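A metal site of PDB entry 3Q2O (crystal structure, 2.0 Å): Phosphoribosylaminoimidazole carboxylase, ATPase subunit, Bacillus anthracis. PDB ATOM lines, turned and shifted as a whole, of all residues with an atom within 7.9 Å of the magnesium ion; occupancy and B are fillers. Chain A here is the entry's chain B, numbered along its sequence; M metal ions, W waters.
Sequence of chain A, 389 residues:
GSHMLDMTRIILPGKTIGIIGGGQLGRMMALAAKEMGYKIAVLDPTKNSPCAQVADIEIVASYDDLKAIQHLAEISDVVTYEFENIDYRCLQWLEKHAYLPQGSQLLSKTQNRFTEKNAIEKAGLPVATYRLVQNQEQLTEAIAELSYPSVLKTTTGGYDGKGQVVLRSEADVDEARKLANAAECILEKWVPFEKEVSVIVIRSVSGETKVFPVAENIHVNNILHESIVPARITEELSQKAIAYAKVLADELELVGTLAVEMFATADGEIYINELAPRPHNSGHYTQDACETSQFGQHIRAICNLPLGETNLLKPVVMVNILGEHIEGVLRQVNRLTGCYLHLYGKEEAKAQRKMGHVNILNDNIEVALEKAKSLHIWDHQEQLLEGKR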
ATOM      1  N   GLU A  84      -8.053  -2.091  36.067  1.00  0.00           N
ATOM      2  CA  GLU A  84      -7.612  -0.967  35.249  1.00  0.00           C
ATOM      3  C   GLU A  84      -8.409   0.320  35.503  1.00  0.00           C
ATOM      4  O   GLU A  84      -7.992   1.403  35.073  1.00  0.00           O
ATOM      5  CB  GLU A  84      -7.686  -1.352  33.774  1.00  0.00           C
ATOM      6  CG  GLU A  84      -6.599  -0.732  32.941  1.00  0.00           C
ATOM      7  CD  GLU A  84      -7.084  -0.353  31.563  1.00  0.00           C
ATOM      8  OE1 GLU A  84      -7.353  -1.265  30.754  1.00  0.00           O
ATOM      9  OE2 GLU A  84      -7.205   0.863  31.309  1.00  0.00           O
ATOM     10  N   LEU A 106       1.269   6.117  33.326  1.00  0.00           N
ATOM     11  CA  LEU A 106       0.772   5.376  32.162  1.00  0.00           C
ATOM     12  C   LEU A 106      -0.691   4.981  32.318  1.00  0.00           C
ATOM     13  O   LEU A 106      -1.459   5.014  31.359  1.00  0.00           O
ATOM     14  CB  LEU A 106       1.634   4.136  31.860  1.00  0.00           C
ATOM     15  CG  LEU A 106       1.185   3.321  30.630  1.00  0.00           C
ATOM     16  CD1 LEU A 106       1.189   4.182  29.362  1.00  0.00           C
ATOM     17  CD2 LEU A 106       2.032   2.105  30.411  1.00  0.00           C
ATOM     18  N   LEU A 107      -1.055   4.604  33.546  1.00  0.00           N
ATOM     19  CA  LEU A 107      -2.434   4.268  33.851  1.00  0.00           C
ATOM     20  C   LEU A 107      -3.341   5.470  33.574  1.00  0.00           C
ATOM     21  O   LEU A 107      -4.368   5.331  32.929  1.00  0.00           O
ATOM     22  CB  LEU A 107      -2.531   3.803  35.318  1.00  0.00           C
ATOM     23  CG  LEU A 107      -3.810   3.162  35.864  1.00  0.00           C
ATOM     24  CD1 LEU A 107      -4.732   4.234  36.430  1.00  0.00           C
ATOM     25  CD2 LEU A 107      -4.537   2.276  34.859  1.00  0.00           C
ATOM     26  N   LYS A 109      -2.827   7.992  31.564  1.00  0.00           N
ATOM     27  CA  LYS A 109      -2.889   8.263  30.134  1.00  0.00           C
ATOM     28  C   LYS A 109      -3.806   7.311  29.373  1.00  0.00           C
ATOM     29  O   LYS A 109      -4.454   7.736  28.401  1.00  0.00           O
ATOM     30  CB  LYS A 109      -1.490   8.248  29.495  1.00  0.00           C
ATOM     31  CG  LYS A 109      -0.654   9.474  29.790  1.00  0.00           C
ATOM     32  CD  LYS A 109       0.727   9.339  29.183  1.00  0.00           C
ATOM     33  CE  LYS A 109       1.646  10.425  29.689  1.00  0.00           C
ATOM     34  NZ  LYS A 109       3.068  10.085  29.393  1.00  0.00           N
ATOM     35  N   THR A 110      -3.874   6.052  29.804  1.00  0.00           N
ATOM     36  CA  THR A 110      -4.565   4.995  29.051  1.00  0.00           C
ATOM     37  C   THR A 110      -5.998   4.728  29.513  1.00  0.00           C
ATOM     38  O   THR A 110      -6.737   3.981  28.851  1.00  0.00           O
ATOM     39  CB  THR A 110      -3.794   3.651  29.101  1.00  0.00           C
ATOM     40  OG1 THR A 110      -3.647   3.238  30.458  1.00  0.00           O
ATOM     41  CG2 THR A 110      -2.434   3.803  28.472  1.00  0.00           C
ATOM     42  N   GLN A 111      -6.372   5.329  30.637  1.00  0.00           N
ATOM     43  CA  GLN A 111      -7.702   5.193  31.231  1.00  0.00           C
ATOM     44  C   GLN A 111      -8.767   5.995  30.504  1.00  0.00           C
ATOM     45  O   GLN A 111      -9.954   5.680  30.568  1.00  0.00           O
ATOM     46  CB  GLN A 111      -7.682   5.706  32.668  1.00  0.00           C
ATOM     47  CG  GLN A 111      -7.442   4.650  33.688  1.00  0.00           C
ATOM     48  CD  GLN A 111      -7.684   5.178  35.090  1.00  0.00           C
ATOM     49  OE1 GLN A 111      -7.392   6.351  35.391  1.00  0.00           O
ATOM     50  NE2 GLN A 111      -8.219   4.327  35.947  1.00  0.00           N
ATOM     51  N   ASN A 112      -8.344   7.070  29.870  1.00  0.00           N
ATOM     52  CA  ASN A 112      -9.257   7.983  29.215  1.00  0.00           C
ATOM     53  C   ASN A 112      -8.948   7.992  27.725  1.00  0.00           C
ATOM     54  O   ASN A 112      -7.842   8.338  27.322  1.00  0.00           O
ATOM     55  CB  ASN A 112      -9.128   9.370  29.844  1.00  0.00           C
ATOM     56  CG  ASN A 112     -10.042  10.388  29.215  1.00  0.00           C
ATOM     57  OD1 ASN A 112      -9.917  10.690  28.032  1.00  0.00           O
ATOM     58  ND2 ASN A 112     -10.972  10.919  29.997  1.00  0.00           N
ATOM     59  N   ARG A 113      -9.926   7.590  26.915  1.00  0.00           N
ATOM     60  CA  ARG A 113      -9.762   7.465  25.462  1.00  0.00           C
ATOM     61  C   ARG A 113      -9.215   8.729  24.776  1.00  0.00           C
ATOM     62  O   ARG A 113      -8.413   8.628  23.850  1.00  0.00           O
ATOM     63  CB  ARG A 113     -11.080   7.020  24.803  1.00  0.00           C
ATOM     64  CG  ARG A 113     -11.333   5.512  24.864  1.00  0.00           C
ATOM     65  CD  ARG A 113     -12.730   5.179  24.365  1.00  0.00           C
ATOM     66  NE  ARG A 113     -12.872   3.823  23.831  1.00  0.00           N
ATOM     67  CZ  ARG A 113     -13.154   2.730  24.548  1.00  0.00           C
ATOM     68  NH1 ARG A 113     -13.331   2.810  25.861  1.00  0.00           N
ATOM     69  NH2 ARG A 113     -13.272   1.553  23.949  1.00  0.00           N
ATOM     70  N   GLU A 116      -5.602   9.167  25.958  1.00  0.00           N
ATOM     71  CA  GLU A 116      -4.943   8.075  25.250  1.00  0.00           C
ATOM     72  C   GLU A 116      -4.565   8.463  23.812  1.00  0.00           C
ATOM     73  O   GLU A 116      -3.415   8.289  23.399  1.00  0.00           O
ATOM     74  CB  GLU A 116      -5.834   6.851  25.245  1.00  0.00           C
ATOM     75  CG  GLU A 116      -5.195   5.595  24.694  1.00  0.00           C
ATOM     76  CD  GLU A 116      -6.057   4.384  24.907  1.00  0.00           C
ATOM     77  OE1 GLU A 116      -5.660   3.524  25.709  1.00  0.00           O
ATOM     78  OE2 GLU A 116      -7.163   4.299  24.323  1.00  0.00           O
ATOM     79  N   THR A 155     -15.338   8.143  26.957  1.00  0.00           N
ATOM     80  CA  THR A 155     -13.910   8.290  27.209  1.00  0.00           C
ATOM     81  C   THR A 155     -13.388   7.373  28.330  1.00  0.00           C
ATOM     82  O   THR A 155     -12.228   6.980  28.303  1.00  0.00           O
ATOM     83  CB  THR A 155     -13.490   9.741  27.502  1.00  0.00           C
ATOM     84  OG1 THR A 155     -14.286  10.285  28.564  1.00  0.00           O
ATOM     85  CG2 THR A 155     -13.627  10.603  26.241  1.00  0.00           C
ATOM     86  N   LEU A 258       2.169  -3.729  28.113  1.00  0.00           N
ATOM     87  CA  LEU A 258       1.266  -2.908  27.344  1.00  0.00           C
ATOM     88  C   LEU A 258       0.669  -3.683  26.165  1.00  0.00           C
ATOM     89  O   LEU A 258       1.389  -4.204  25.322  1.00  0.00           O
ATOM     90  CB  LEU A 258       1.983  -1.631  26.862  1.00  0.00           C
ATOM     91  CG  LEU A 258       1.171  -0.594  26.083  1.00  0.00           C
ATOM     92  CD1 LEU A 258       0.239   0.206  27.015  1.00  0.00           C
ATOM     93  CD2 LEU A 258       2.125   0.338  25.342  1.00  0.00           C
ATOM     94  N   ALA A 259      -0.664  -3.735  26.140  1.00  0.00           N
ATOM     95  CA  ALA A 259      -1.403  -4.348  25.050  1.00  0.00           C
ATOM     96  C   ALA A 259      -1.829  -3.235  24.079  1.00  0.00           C
ATOM     97  O   ALA A 259      -2.508  -2.275  24.482  1.00  0.00           O
ATOM     98  CB  ALA A 259      -2.633  -5.053  25.592  1.00  0.00           C
ATOM     99  N   GLU A 261      -3.903  -2.502  20.769  1.00  0.00           N
ATOM    100  CA  GLU A 261      -4.891  -2.946  19.789  1.00  0.00           C
ATOM    101  C   GLU A 261      -4.856  -2.031  18.574  1.00  0.00           C
ATOM    102  O   GLU A 261      -4.698  -0.806  18.716  1.00  0.00           O
ATOM    103  CB  GLU A 261      -6.300  -3.008  20.395  1.00  0.00           C
ATOM    104  CG  GLU A 261      -6.397  -3.971  21.597  1.00  0.00           C
ATOM    105  CD  GLU A 261      -7.831  -4.185  22.066  1.00  0.00           C
ATOM    106  OE1 GLU A 261      -8.211  -3.584  23.088  1.00  0.00           O
ATOM    107  OE2 GLU A 261      -8.575  -4.944  21.422  1.00  0.00           O
ATOM    108  N   ASN A 273      -5.727   1.626  17.872  1.00  0.00           N
ATOM    109  CA  ASN A 273      -7.107   1.672  18.364  1.00  0.00           C
ATOM    110  C   ASN A 273      -7.157   2.073  19.848  1.00  0.00           C
ATOM    111  O   ASN A 273      -7.642   3.153  20.177  1.00  0.00           O
ATOM    112  CB  ASN A 273      -7.778   0.325  18.120  1.00  0.00           C
ATOM    113  CG  ASN A 273      -9.191   0.225  18.700  1.00  0.00           C
ATOM    114  OD1 ASN A 273      -9.916   1.226  18.809  1.00  0.00           O
ATOM    115  ND2 ASN A 273      -9.605  -0.992  19.020  1.00  0.00           N
ATOM    116  N   GLU A 274      -6.676   1.188  20.716  1.00  0.00           N
ATOM    117  CA  GLU A 274      -6.537   1.514  22.128  1.00  0.00           C
ATOM    118  C   GLU A 274      -5.419   0.731  22.813  1.00  0.00           C
ATOM    119  O   GLU A 274      -4.848  -0.195  22.231  1.00  0.00           O
ATOM    120  CB  GLU A 274      -7.869   1.392  22.886  1.00  0.00           C
ATOM    121  CG  GLU A 274      -8.604   0.060  22.759  1.00  0.00           C
ATOM    122  CD  GLU A 274      -9.907   0.063  23.548  1.00  0.00           C
ATOM    123  OE1 GLU A 274     -10.952   0.434  22.974  1.00  0.00           O
ATOM    124  OE2 GLU A 274      -9.892  -0.267  24.751  1.00  0.00           O
ATOM    125  N   LEU A 275      -5.107   1.141  24.042  1.00  0.00           N
ATOM    126  CA  LEU A 275      -4.004   0.620  24.824  1.00  0.00           C
ATOM    127  C   LEU A 275      -4.509   0.125  26.172  1.00  0.00           C
ATOM    128  O   LEU A 275      -5.477   0.670  26.729  1.00  0.00           O
ATOM    129  CB  LEU A 275      -2.979   1.723  25.069  1.00  0.00           C
ATOM    130  CG  LEU A 275      -2.439   2.496  23.855  1.00  0.00           C
ATOM    131  CD1 LEU A 275      -1.508   3.606  24.326  1.00  0.00           C
ATOM    132  CD2 LEU A 275      -1.734   1.560  22.860  1.00  0.00           C
ATOM    133  N   ALA A 276      -3.857  -0.907  26.691  1.00  0.00           N
ATOM    134  CA  ALA A 276      -4.174  -1.422  28.026  1.00  0.00           C
ATOM    135  C   ALA A 276      -2.874  -1.656  28.778  1.00  0.00           C
ATOM    136  O   ALA A 276      -2.020  -2.414  28.322  1.00  0.00           O
ATOM    137  CB  ALA A 276      -5.024  -2.712  27.934  1.00  0.00           C
ATOM    138  N   PRO A 277      -2.699  -0.987  29.919  1.00  0.00           N
ATOM    139  CA  PRO A 277      -1.437  -1.082  30.656  1.00  0.00           C
ATOM    140  C   PRO A 277      -1.375  -2.346  31.537  1.00  0.00           C
ATOM    141  O   PRO A 277      -1.102  -2.265  32.735  1.00  0.00           O
ATOM    142  CB  PRO A 277      -1.433   0.210  31.483  1.00  0.00           C
ATOM    143  CG  PRO A 277      -2.869   0.462  31.755  1.00  0.00           C
ATOM    144  CD  PRO A 277      -3.649  -0.076  30.591  1.00  0.00           C
ATOM    145  N   ARG A 278      -1.619  -3.514  30.927  1.00  0.00           N
ATOM    146  CA  ARG A 278      -1.745  -4.774  31.667  1.00  0.00           C
ATOM    147  C   ARG A 278      -1.825  -5.953  30.697  1.00  0.00           C
ATOM    148  O   ARG A 278      -2.075  -5.769  29.498  1.00  0.00           O
ATOM    149  CB  ARG A 278      -3.028  -4.770  32.519  1.00  0.00           C
ATOM    150  CG  ARG A 278      -4.239  -4.272  31.743  1.00  0.00           C
ATOM    151  CD  ARG A 278      -5.573  -4.677  32.317  1.00  0.00           C
ATOM    152  NE  ARG A 278      -6.643  -4.189  31.463  1.00  0.00           N
ATOM    153  CZ  ARG A 278      -7.136  -4.831  30.405  1.00  0.00           C
ATOM    154  NH1 ARG A 278      -6.666  -6.030  30.038  1.00  0.00           N
ATOM    155  NH2 ARG A 278      -8.120  -4.275  29.702  1.00  0.00           N
HETATM  156 MG    MG M   1      -7.142   2.211  27.183  1.00  0.00          MG
HETATM  157  O   HOH W   1      -7.602   0.900  28.632  1.00  0.00           O
HETATM  158  O   HOH W   2      -8.814   3.033  26.152  1.00  0.00           O
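The nearest printed residue that does not touch the magnesium ion is Glu 84 (4.3 Å).
The magnesium ion is bound by water W1, at 2.0 Å.
Water W2 binds the magnesium ion.
O of Leu 275 is bound to the magnesium ion (2.3 Å).
O of Thr 110 is bound to the magnesium ion (2.5 Å).
OE1 of Glu 116 binds the magnesium ion, at 2.5 Å.
The magnesium ion has five donor atoms within binding distance.
The backbone carbonyl oxygen (O) of Leu 107 lies within hydrogen-bond range of the side-chain hydroxyl (OG1) of Thr 110 (3.3 Å).
The side-chain hydroxyl of Thr 110 lies within hydrogen-bond range of the backbone carbonyl oxygen of Leu 106.
O of Lys 109 sits at hydrogen-bond distance from N of Glu 116, 3.1 Å away.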
